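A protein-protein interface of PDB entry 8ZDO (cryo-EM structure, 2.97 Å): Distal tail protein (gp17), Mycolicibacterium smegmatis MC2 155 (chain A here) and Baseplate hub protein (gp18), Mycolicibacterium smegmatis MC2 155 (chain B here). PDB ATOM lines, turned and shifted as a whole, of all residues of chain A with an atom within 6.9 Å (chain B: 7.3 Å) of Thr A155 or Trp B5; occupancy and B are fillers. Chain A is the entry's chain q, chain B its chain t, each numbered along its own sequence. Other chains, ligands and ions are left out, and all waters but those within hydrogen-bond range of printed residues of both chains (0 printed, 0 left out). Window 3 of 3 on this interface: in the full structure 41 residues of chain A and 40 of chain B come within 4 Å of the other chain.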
ATOM      1  N   ILE A 153      30.388  12.649  -1.949  1.00  0.00           N
ATOM      2  CA  ILE A 153      29.306  12.830  -0.990  1.00  0.00           C
ATOM      3  C   ILE A 153      28.423  13.981  -1.446  1.00  0.00           C
ATOM      4  O   ILE A 153      28.923  15.034  -1.858  1.00  0.00           O
ATOM      5  CB  ILE A 153      29.843  13.094   0.432  1.00  0.00           C
ATOM      6  CG1 ILE A 153      30.636  11.891   0.938  1.00  0.00           C
ATOM      7  CG2 ILE A 153      28.706  13.408   1.385  1.00  0.00           C
ATOM      8  CD1 ILE A 153      31.011  11.986   2.390  1.00  0.00           C
ATOM      9  N   TRP A 154      27.109  13.779  -1.376  1.00  0.00           N
ATOM     10  CA  TRP A 154      26.129  14.820  -1.660  1.00  0.00           C
ATOM     11  C   TRP A 154      25.063  14.782  -0.576  1.00  0.00           C
ATOM     12  O   TRP A 154      24.272  13.837  -0.515  1.00  0.00           O
ATOM     13  CB  TRP A 154      25.502  14.634  -3.038  1.00  0.00           C
ATOM     14  CG  TRP A 154      24.314  15.512  -3.268  1.00  0.00           C
ATOM     15  CD1 TRP A 154      24.325  16.847  -3.538  1.00  0.00           C
ATOM     16  CD2 TRP A 154      22.939  15.118  -3.243  1.00  0.00           C
ATOM     17  NE1 TRP A 154      23.042  17.309  -3.687  1.00  0.00           N
ATOM     18  CE2 TRP A 154      22.172  16.266  -3.511  1.00  0.00           C
ATOM     19  CE3 TRP A 154      22.283  13.904  -3.025  1.00  0.00           C
ATOM     20  CZ2 TRP A 154      20.784  16.237  -3.565  1.00  0.00           C
ATOM     21  CZ3 TRP A 154      20.904  13.880  -3.079  1.00  0.00           C
ATOM     22  CH2 TRP A 154      20.169  15.038  -3.347  1.00  0.00           C
ATOM     23  N   THR A 155      25.042  15.796   0.277  1.00  0.00           N
ATOM     24  CA  THR A 155      24.024  15.931   1.304  1.00  0.00           C
ATOM     25  C   THR A 155      23.068  17.051   0.922  1.00  0.00           C
ATOM     26  O   THR A 155      23.436  17.975   0.192  1.00  0.00           O
ATOM     27  CB  THR A 155      24.646  16.217   2.673  1.00  0.00           C
ATOM     28  OG1 THR A 155      23.607  16.428   3.635  1.00  0.00           O
ATOM     29  CG2 THR A 155      25.531  17.449   2.610  1.00  0.00           C
ATOM     30  N   THR A 156      21.833  16.962   1.407  1.00  0.00           N
ATOM     31  CA  THR A 156      20.859  17.996   1.096  1.00  0.00           C
ATOM     32  C   THR A 156      19.891  18.147   2.257  1.00  0.00           C
ATOM     33  O   THR A 156      19.757  17.260   3.104  1.00  0.00           O
ATOM     34  CB  THR A 156      20.095  17.686  -0.197  1.00  0.00           C
ATOM     35  OG1 THR A 156      19.386  18.854  -0.626  1.00  0.00           O
ATOM     36  CG2 THR A 156      19.105  16.558   0.022  1.00  0.00           C
ATOM     37  N   LEU A 157      19.224  19.298   2.290  1.00  0.00           N
ATOM     38  CA  LEU A 157      18.165  19.558   3.249  1.00  0.00           C
ATOM     39  C   LEU A 157      16.786  19.598   2.611  1.00  0.00           C
ATOM     40  O   LEU A 157      15.787  19.602   3.337  1.00  0.00           O
ATOM     41  CB  LEU A 157      18.419  20.886   3.980  1.00  0.00           C
ATOM     42  CG  LEU A 157      19.523  20.890   5.039  1.00  0.00           C
ATOM     43  CD1 LEU A 157      20.867  21.226   4.416  1.00  0.00           C
ATOM     44  CD2 LEU A 157      19.189  21.864   6.156  1.00  0.00           C
ATOM     45  N   SER A 158      16.707  19.628   1.284  1.00  0.00           N
ATOM     46  CA  SER A 158      15.425  19.715   0.605  1.00  0.00           C
ATOM     47  C   SER A 158      14.670  18.395   0.699  1.00  0.00           C
ATOM     48  O   SER A 158      15.263  17.318   0.785  1.00  0.00           O
ATOM     49  CB  SER A 158      15.624  20.092  -0.863  1.00  0.00           C
ATOM     50  OG  SER A 158      16.248  21.356  -0.987  1.00  0.00           O
ATOM     51  N   ASP A 161      15.168  16.565  -4.207  1.00  0.00           N
ATOM     52  CA  ASP A 161      16.366  17.141  -4.803  1.00  0.00           C
ATOM     53  C   ASP A 161      16.970  16.150  -5.789  1.00  0.00           C
ATOM     54  O   ASP A 161      16.564  14.990  -5.869  1.00  0.00           O
ATOM     55  CB  ASP A 161      17.386  17.534  -3.732  1.00  0.00           C
ATOM     56  CG  ASP A 161      18.214  18.737  -4.134  1.00  0.00           C
ATOM     57  OD1 ASP A 161      18.166  19.118  -5.320  1.00  0.00           O
ATOM     58  OD2 ASP A 161      18.911  19.301  -3.265  1.00  0.00           O
ATOM     59  N   PHE A 165      26.687  12.896 -10.136  1.00  0.00           N
ATOM     60  CA  PHE A 165      27.999  12.451  -9.701  1.00  0.00           C
ATOM     61  C   PHE A 165      28.875  12.213 -10.917  1.00  0.00           C
ATOM     62  O   PHE A 165      28.510  11.389 -11.768  1.00  0.00           O
ATOM     63  CB  PHE A 165      27.888  11.173  -8.884  1.00  0.00           C
ATOM     64  CG  PHE A 165      27.470  11.390  -7.463  1.00  0.00           C
ATOM     65  CD1 PHE A 165      28.339  11.953  -6.550  1.00  0.00           C
ATOM     66  CD2 PHE A 165      26.211  11.015  -7.036  1.00  0.00           C
ATOM     67  CE1 PHE A 165      27.956  12.145  -5.242  1.00  0.00           C
ATOM     68  CE2 PHE A 165      25.825  11.204  -5.730  1.00  0.00           C
ATOM     69  CZ  PHE A 165      26.698  11.769  -4.832  1.00  0.00           C
ATOM     70  N   THR A 182      21.039   7.635   3.080  1.00  0.00           N
ATOM     71  CA  THR A 182      20.412   7.802   4.382  1.00  0.00           C
ATOM     72  C   THR A 182      18.894   7.646   4.278  1.00  0.00           C
ATOM     73  O   THR A 182      18.316   7.596   3.192  1.00  0.00           O
ATOM     74  CB  THR A 182      20.766   9.157   4.990  1.00  0.00           C
ATOM     75  OG1 THR A 182      20.124  10.194   4.248  1.00  0.00           O
ATOM     76  CG2 THR A 182      22.264   9.371   4.967  1.00  0.00           C
ATOM     77  N   ALA A 183      18.253   7.568   5.436  1.00  0.00           N
ATOM     78  CA  ALA A 183      16.818   7.379   5.570  1.00  0.00           C
ATOM     79  C   ALA A 183      16.257   8.419   6.524  1.00  0.00           C
ATOM     80  O   ALA A 183      16.979   8.930   7.387  1.00  0.00           O
ATOM     81  CB  ALA A 183      16.499   5.970   6.087  1.00  0.00           C
ATOM     82  N   PRO A 184      14.965   8.761   6.401  1.00  0.00           N
ATOM     83  CA  PRO A 184      13.965   8.285   5.431  1.00  0.00           C
ATOM     84  C   PRO A 184      14.191   8.852   4.041  1.00  0.00           C
ATOM     85  O   PRO A 184      15.030   9.723   3.845  1.00  0.00           O
ATOM     86  CB  PRO A 184      12.635   8.793   6.017  1.00  0.00           C
ATOM     87  CG  PRO A 184      12.924   9.116   7.449  1.00  0.00           C
ATOM     88  CD  PRO A 184      14.340   9.596   7.435  1.00  0.00           C
ATOM     89  N   HIS A 220      19.111   3.410   7.146  1.00  0.00           N
ATOM     90  CA  HIS A 220      20.168   3.781   6.218  1.00  0.00           C
ATOM     91  C   HIS A 220      20.689   2.533   5.523  1.00  0.00           C
ATOM     92  O   HIS A 220      20.970   1.524   6.174  1.00  0.00           O
ATOM     93  CB  HIS A 220      21.295   4.500   6.952  1.00  0.00           C
ATOM     94  CG  HIS A 220      20.813   5.505   7.948  1.00  0.00           C
ATOM     95  ND1 HIS A 220      20.084   6.615   7.590  1.00  0.00           N
ATOM     96  CD2 HIS A 220      20.954   5.565   9.293  1.00  0.00           C
ATOM     97  CE1 HIS A 220      19.795   7.317   8.670  1.00  0.00           C
ATOM     98  NE2 HIS A 220      20.312   6.701   9.716  1.00  0.00           N
ATOM     99  N   GLU A 270      13.413  15.182   6.338  1.00  0.00           N
ATOM    100  CA  GLU A 270      14.624  15.752   6.916  1.00  0.00           C
ATOM    101  C   GLU A 270      15.578  16.260   5.842  1.00  0.00           C
ATOM    102  O   GLU A 270      16.240  17.286   6.030  1.00  0.00           O
ATOM    103  CB  GLU A 270      15.327  14.717   7.793  1.00  0.00           C
ATOM    104  CG  GLU A 270      14.639  14.448   9.120  1.00  0.00           C
ATOM    105  CD  GLU A 270      13.678  13.281   9.048  1.00  0.00           C
ATOM    106  OE1 GLU A 270      13.483  12.737   7.941  1.00  0.00           O
ATOM    107  OE2 GLU A 270      13.119  12.904  10.099  1.00  0.00           O
ATOM    108  N   GLY A 271      15.659  15.560   4.715  1.00  0.00           N
ATOM    109  CA  GLY A 271      16.673  15.844   3.722  1.00  0.00           C
ATOM    110  C   GLY A 271      17.879  14.968   3.967  1.00  0.00           C
ATOM    111  O   GLY A 271      18.572  15.127   4.977  1.00  0.00           O
ATOM    112  N   GLY A 272      18.149  14.036   3.053  1.00  0.00           N
ATOM    113  CA  GLY A 272      19.105  12.980   3.287  1.00  0.00           C
ATOM    114  C   GLY A 272      20.468  13.240   2.671  1.00  0.00           C
ATOM    115  O   GLY A 272      20.763  14.312   2.137  1.00  0.00           O
ATOM    116  N   ALA A 273      21.308  12.212   2.747  1.00  0.00           N
ATOM    117  CA  ALA A 273      22.653  12.252   2.202  1.00  0.00           C
ATOM    118  C   ALA A 273      22.930  10.989   1.398  1.00  0.00           C
ATOM    119  O   ALA A 273      22.385   9.911   1.673  1.00  0.00           O
ATOM    120  CB  ALA A 273      23.698  12.407   3.306  1.00  0.00           C
ATOM    121  N   CYS A 274      23.794  11.146   0.400  1.00  0.00           N
ATOM    122  CA  CYS A 274      24.204  10.084  -0.498  1.00  0.00           C
ATOM    123  C   CYS A 274      25.721  10.054  -0.580  1.00  0.00           C
ATOM    124  O   CYS A 274      26.379  11.096  -0.582  1.00  0.00           O
ATOM    125  CB  CYS A 274      23.616  10.284  -1.901  1.00  0.00           C
ATOM    126  SG  CYS A 274      24.046   9.009  -3.103  1.00  0.00           S
ATOM    127  N   ALA B   2      16.449   4.266  15.495  1.00  0.00           N
ATOM    128  CA  ALA B   2      16.251   5.215  14.405  1.00  0.00           C
ATOM    129  C   ALA B   2      17.229   6.377  14.509  1.00  0.00           C
ATOM    130  O   ALA B   2      16.862   7.476  14.921  1.00  0.00           O
ATOM    131  CB  ALA B   2      14.819   5.726  14.400  1.00  0.00           C
ATOM    132  N   ASN B   3      18.480   6.125  14.131  1.00  0.00           N
ATOM    133  CA  ASN B   3      19.510   7.157  14.142  1.00  0.00           C
ATOM    134  C   ASN B   3      19.398   7.970  12.860  1.00  0.00           C
ATOM    135  O   ASN B   3      19.742   7.485  11.778  1.00  0.00           O
ATOM    136  CB  ASN B   3      20.892   6.528  14.275  1.00  0.00           C
ATOM    137  CG  ASN B   3      21.092   5.841  15.610  1.00  0.00           C
ATOM    138  OD1 ASN B   3      21.158   4.614  15.685  1.00  0.00           O
ATOM    139  ND2 ASN B   3      21.193   6.630  16.671  1.00  0.00           N
ATOM    140  N   ASN B   4      18.916   9.204  12.975  1.00  0.00           N
ATOM    141  CA  ASN B   4      18.758  10.047  11.804  1.00  0.00           C
ATOM    142  C   ASN B   4      20.118  10.490  11.275  1.00  0.00           C
ATOM    143  O   ASN B   4      21.147  10.369  11.946  1.00  0.00           O
ATOM    144  CB  ASN B   4      17.904  11.270  12.132  1.00  0.00           C
ATOM    145  CG  ASN B   4      16.514  10.899  12.599  1.00  0.00           C
ATOM    146  OD1 ASN B   4      15.995   9.839  12.249  1.00  0.00           O
ATOM    147  ND2 ASN B   4      15.902  11.770  13.391  1.00  0.00           N
ATOM    148  N   TRP B   5      20.114  11.002  10.043  1.00  0.00           N
ATOM    149  CA  TRP B   5      21.353  11.499   9.459  1.00  0.00           C
ATOM    150  C   TRP B   5      21.907  12.669  10.258  1.00  0.00           C
ATOM    151  O   TRP B   5      23.120  12.763  10.471  1.00  0.00           O
ATOM    152  CB  TRP B   5      21.137  11.912   8.005  1.00  0.00           C
ATOM    153  CG  TRP B   5      22.284  12.704   7.472  1.00  0.00           C
ATOM    154  CD1 TRP B   5      22.277  14.017   7.118  1.00  0.00           C
ATOM    155  CD2 TRP B   5      23.619  12.237   7.257  1.00  0.00           C
ATOM    156  NE1 TRP B   5      23.524  14.398   6.688  1.00  0.00           N
ATOM    157  CE2 TRP B   5      24.366  13.321   6.764  1.00  0.00           C
ATOM    158  CE3 TRP B   5      24.256  11.004   7.429  1.00  0.00           C
ATOM    159  CZ2 TRP B   5      25.713  13.211   6.440  1.00  0.00           C
ATOM    160  CZ3 TRP B   5      25.591  10.898   7.107  1.00  0.00           C
ATOM    161  CH2 TRP B   5      26.307  11.994   6.619  1.00  0.00           C
ATOM    162  N   THR B   6      21.035  13.576  10.702  1.00  0.00           N
ATOM    163  CA  THR B   6      21.492  14.701  11.512  1.00  0.00           C
ATOM    164  C   THR B   6      22.089  14.221  12.828  1.00  0.00           C
ATOM    165  O   THR B   6      23.113  14.742  13.281  1.00  0.00           O
ATOM    166  CB  THR B   6      20.340  15.670  11.769  1.00  0.00           C
ATOM    167  OG1 THR B   6      19.674  15.964  10.536  1.00  0.00           O
ATOM    168  CG2 THR B   6      20.863  16.963  12.366  1.00  0.00           C
ATOM    169  N   ASP B   7      21.462  13.222  13.452  1.00  0.00           N
ATOM    170  CA  ASP B   7      21.988  12.680  14.700  1.00  0.00           C
ATOM    171  C   ASP B   7      23.348  12.026  14.491  1.00  0.00           C
ATOM    172  O   ASP B   7      24.265  12.208  15.302  1.00  0.00           O
ATOM    173  CB  ASP B   7      20.995  11.678  15.285  1.00  0.00           C
ATOM    174  CG  ASP B   7      19.647  12.302  15.580  1.00  0.00           C
ATOM    175  OD1 ASP B   7      19.605  13.513  15.876  1.00  0.00           O
ATOM    176  OD2 ASP B   7      18.630  11.582  15.508  1.00  0.00           O
ATOM    177  N   ILE B   8      23.499  11.259  13.409  1.00  0.00           N
ATOM    178  CA  ILE B   8      24.778  10.613  13.125  1.00  0.00           C
ATOM    179  C   ILE B   8      25.852  11.657  12.846  1.00  0.00           C
ATOM    180  O   ILE B   8      26.994  11.538  13.307  1.00  0.00           O
ATOM    181  CB  ILE B   8      24.629   9.622  11.957  1.00  0.00           C
ATOM    182  CG1 ILE B   8      23.722   8.461  12.359  1.00  0.00           C
ATOM    183  CG2 ILE B   8      25.980   9.095  11.529  1.00  0.00           C
ATOM    184  CD1 ILE B   8      23.460   7.484  11.243  1.00  0.00           C
ATOM    185  N   LEU B   9      25.503  12.698  12.087  1.00  0.00           N
ATOM    186  CA  LEU B   9      26.459  13.762  11.803  1.00  0.00           C
ATOM    187  C   LEU B   9      26.873  14.488  13.076  1.00  0.00           C
ATOM    188  O   LEU B   9      28.048  14.825  13.254  1.00  0.00           O
ATOM    189  CB  LEU B   9      25.862  14.739  10.794  1.00  0.00           C
ATOM    190  CG  LEU B   9      26.856  15.547   9.965  1.00  0.00           C
ATOM    191  CD1 LEU B   9      27.946  14.644   9.430  1.00  0.00           C
ATOM    192  CD2 LEU B   9      26.139  16.253   8.833  1.00  0.00           C
ATOM    193  N   ALA B  10      25.919  14.742  13.974  1.00  0.00           N
ATOM    194  CA  ALA B  10      26.248  15.379  15.245  1.00  0.00           C
ATOM    195  C   ALA B  10      27.158  14.492  16.085  1.00  0.00           C
ATOM    196  O   ALA B  10      28.097  14.979  16.722  1.00  0.00           O
ATOM    197  CB  ALA B  10      24.970  15.716  16.010  1.00  0.00           C
ATOM    198  N   ALA B  11      26.891  13.184  16.102  1.00  0.00           N
ATOM    199  CA  ALA B  11      27.763  12.262  16.821  1.00  0.00           C
ATOM    200  C   ALA B  11      29.164  12.251  16.225  1.00  0.00           C
ATOM    201  O   ALA B  11      30.156  12.124  16.950  1.00  0.00           O
ATOM    202  CB  ALA B  11      27.165  10.857  16.811  1.00  0.00           C
ATOM    203  N   SER B  12      29.265  12.384  14.905  1.00  0.00           N
ATOM    204  CA  SER B  12      30.556  12.441  14.232  1.00  0.00           C
ATOM    205  C   SER B  12      31.148  13.841  14.208  1.00  0.00           C
ATOM    206  O   SER B  12      32.204  14.036  13.597  1.00  0.00           O
ATOM    207  CB  SER B  12      30.425  11.911  12.804  1.00  0.00           C
ATOM    208  OG  SER B  12      29.954  10.575  12.807  1.00  0.00           O
ATOM    209  N   ASP B  15      31.349  15.772  10.572  1.00  0.00           N
ATOM    210  CA  ASP B  15      32.199  15.212   9.529  1.00  0.00           C
ATOM    211  C   ASP B  15      31.384  14.198   8.734  1.00  0.00           C
ATOM    212  O   ASP B  15      31.068  13.112   9.232  1.00  0.00           O
ATOM    213  CB  ASP B  15      33.449  14.574  10.126  1.00  0.00           C
ATOM    214  CG  ASP B  15      34.571  14.448   9.118  1.00  0.00           C
ATOM    215  OD1 ASP B  15      34.367  14.837   7.950  1.00  0.00           O
ATOM    216  OD2 ASP B  15      35.661  13.967   9.496  1.00  0.00           O
ATOM    217  N   GLU B  16      31.048  14.562   7.494  1.00  0.00           N
ATOM    218  CA  GLU B  16      30.245  13.685   6.652  1.00  0.00           C
ATOM    219  C   GLU B  16      30.972  12.380   6.366  1.00  0.00           C
ATOM    220  O   GLU B  16      30.352  11.313   6.322  1.00  0.00           O
ATOM    221  CB  GLU B  16      29.886  14.394   5.349  1.00  0.00           C
ATOM    222  CG  GLU B  16      28.571  15.149   5.393  1.00  0.00           C
ATOM    223  CD  GLU B  16      28.737  16.574   5.882  1.00  0.00           C
ATOM    224  OE1 GLU B  16      29.893  17.010   6.061  1.00  0.00           O
ATOM    225  OE2 GLU B  16      27.712  17.259   6.083  1.00  0.00           O
ATOM    226  N   TRP B  17      32.287  12.448   6.153  1.00  0.00           N
ATOM    227  CA  TRP B  17      33.053  11.237   5.886  1.00  0.00           C
ATOM    228  C   TRP B  17      33.054  10.304   7.090  1.00  0.00           C
ATOM    229  O   TRP B  17      32.903   9.087   6.942  1.00  0.00           O
ATOM    230  CB  TRP B  17      34.476  11.609   5.476  1.00  0.00           C
ATOM    231  CG  TRP B  17      34.498  12.517   4.295  1.00  0.00           C
ATOM    232  CD1 TRP B  17      34.541  13.877   4.308  1.00  0.00           C
ATOM    233  CD2 TRP B  17      34.451  12.131   2.918  1.00  0.00           C
ATOM    234  NE1 TRP B  17      34.533  14.364   3.025  1.00  0.00           N
ATOM    235  CE2 TRP B  17      34.477  13.311   2.153  1.00  0.00           C
ATOM    236  CE3 TRP B  17      34.391  10.901   2.259  1.00  0.00           C
ATOM    237  CZ2 TRP B  17      34.449  13.297   0.763  1.00  0.00           C
ATOM    238  CZ3 TRP B  17      34.363  10.889   0.882  1.00  0.00           C
ATOM    239  CH2 TRP B  17      34.392  12.078   0.149  1.00  0.00           C
ATOM    240  N   ALA B  18      33.208  10.859   8.294  1.00  0.00           N
ATOM    241  CA  ALA B  18      33.138  10.038   9.497  1.00  0.00           C
ATOM    242  C   ALA B  18      31.756   9.419   9.664  1.00  0.00           C
ATOM    243  O   ALA B  18      31.635   8.240  10.019  1.00  0.00           O
ATOM    244  CB  ALA B  18      33.504  10.874  10.722  1.00  0.00           C
ATOM    245  N   ALA B  19      30.702  10.196   9.415  1.00  0.00           N
ATOM    246  CA  ALA B  19      29.349   9.662   9.544  1.00  0.00           C
ATOM    247  C   ALA B  19      29.097   8.536   8.548  1.00  0.00           C
ATOM    248  O   ALA B  19      28.509   7.500   8.892  1.00  0.00           O
ATOM    249  CB  ALA B  19      28.330  10.785   9.356  1.00  0.00           C
ATOM    250  N   PHE B  20      29.543   8.715   7.308  1.00  0.00           N
ATOM    251  CA  PHE B  20      29.343   7.674   6.310  1.00  0.00           C
ATOM    252  C   PHE B  20      30.199   6.451   6.599  1.00  0.00           C
ATOM    253  O   PHE B  20      29.785   5.331   6.295  1.00  0.00           O
ATOM    254  CB  PHE B  20      29.623   8.225   4.916  1.00  0.00           C
ATOM    255  CG  PHE B  20      28.420   8.836   4.265  1.00  0.00           C
ATOM    256  CD1 PHE B  20      27.280   8.085   4.051  1.00  0.00           C
ATOM    257  CD2 PHE B  20      28.423  10.160   3.878  1.00  0.00           C
ATOM    258  CE1 PHE B  20      26.171   8.641   3.456  1.00  0.00           C
ATOM    259  CE2 PHE B  20      27.318  10.722   3.285  1.00  0.00           C
ATOM    260  CZ  PHE B  20      26.191   9.961   3.072  1.00  0.00           C
ATOM    261  N   LYS B  21      31.377   6.634   7.199  1.00  0.00           N
ATOM    262  CA  LYS B  21      32.160   5.479   7.627  1.00  0.00           C
ATOM    263  C   LYS B  21      31.461   4.730   8.753  1.00  0.00           C
ATOM    264  O   LYS B  21      31.515   3.499   8.814  1.00  0.00           O
ATOM    265  CB  LYS B  21      33.559   5.912   8.052  1.00  0.00           C
ATOM    266  CG  LYS B  21      34.573   5.837   6.926  1.00  0.00           C
ATOM    267  CD  LYS B  21      35.923   6.386   7.338  1.00  0.00           C
ATOM    268  CE  LYS B  21      36.888   6.396   6.164  1.00  0.00           C
ATOM    269  NZ  LYS B  21      36.995   7.742   5.534  1.00  0.00           N
ATOM    270  N   ILE B  23      28.169   4.528   9.084  1.00  0.00           N
ATOM    271  CA  ILE B  23      27.095   3.791   8.419  1.00  0.00           C
ATOM    272  C   ILE B  23      27.653   2.578   7.681  1.00  0.00           C
ATOM    273  O   ILE B  23      27.056   1.492   7.694  1.00  0.00           O
ATOM    274  CB  ILE B  23      26.317   4.726   7.475  1.00  0.00           C
ATOM    275  CG1 ILE B  23      25.726   5.893   8.263  1.00  0.00           C
ATOM    276  CG2 ILE B  23      25.228   3.963   6.739  1.00  0.00           C
ATOM    277  CD1 ILE B  23      24.875   6.817   7.435  1.00  0.00           C
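The side-chain hydroxyl (OG1) of Thr A182 lies within hydrogen-bond range of the backbone NH (N) of Ala A273, 2.8 Å away.
The backbone carbonyl oxygen (O) of Trp A154 sits at hydrogen-bond distance from the backbone NH (N) of Cys A274.
O of Ile B8 sits at hydrogen-bond distance from OG of Ser B12.
The backbone NH of Ala A183 lies within hydrogen-bond range of a ring nitrogen (ND1) of His A220 (3.0 Å).
Thr A155 touches just one residue of chain B: Trp B5 (3.7 Å).
Printed residues of chain A within 4 Å of Trp B5: Thr A155 (3.7 Å), Thr A182 (3.6 Å), His A220 (3.9 Å) and Ala A273 (3.6 Å).
Printed residues of chain B within 4 Å of His A220: Asn B3 (2.3 Å), Trp B5 (3.9 Å), Ile B8 (3.6 Å) and Ile B23 (3.98 Å).
Of the printed residues of chain A, Phe B20 touches Ile A153 (3.5 Å), Ala A273 (3.5 Å) and Cys A274 (3.7 Å).
Printed residues of chain A within 4 Å of Trp B17: Ile A153 (3.5 Å).
The nearest residue of chain B that does not touch Thr A155 is Glu B16 (4.1 Å).
The nearest residue of chain A that does not touch Trp B5 is Gly A271 (4.4 Å).
Hydrophobic or aromatic side chains of chain A within 4 Å of the printed part of chain B: Ile A153, His A220 and Ala A273.
Among the printed residues, no Asp or Glu carboxylate lies within 4 Å of a Lys or Arg side-chain nitrogen of the other chain.
Among the printed residues, merely in contact across the chains: Ile A153 with Glu B16 (3.98 Å), Ile A153 with Trp B17 (3.5 Å), Ile A153 with Phe B20 (3.5 Å), Thr A155 with Trp B5 (3.7 Å), Thr A182 with Trp B5 (3.6 Å), His A220 with Trp B5 (3.9 Å), His A220 with Ile B8 (3.6 Å), His A220 with Ile B23 (3.98 Å), Ala A273 with Trp B5 (3.6 Å), Ala A273 with Phe B20 (3.5 Å) and Cys A274 with Phe B20 (3.7 Å).
A ring nitrogen (NE2) of His A220 lies close to the backbone carbonyl oxygen (O) of Asn B3 (2.3 Å).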
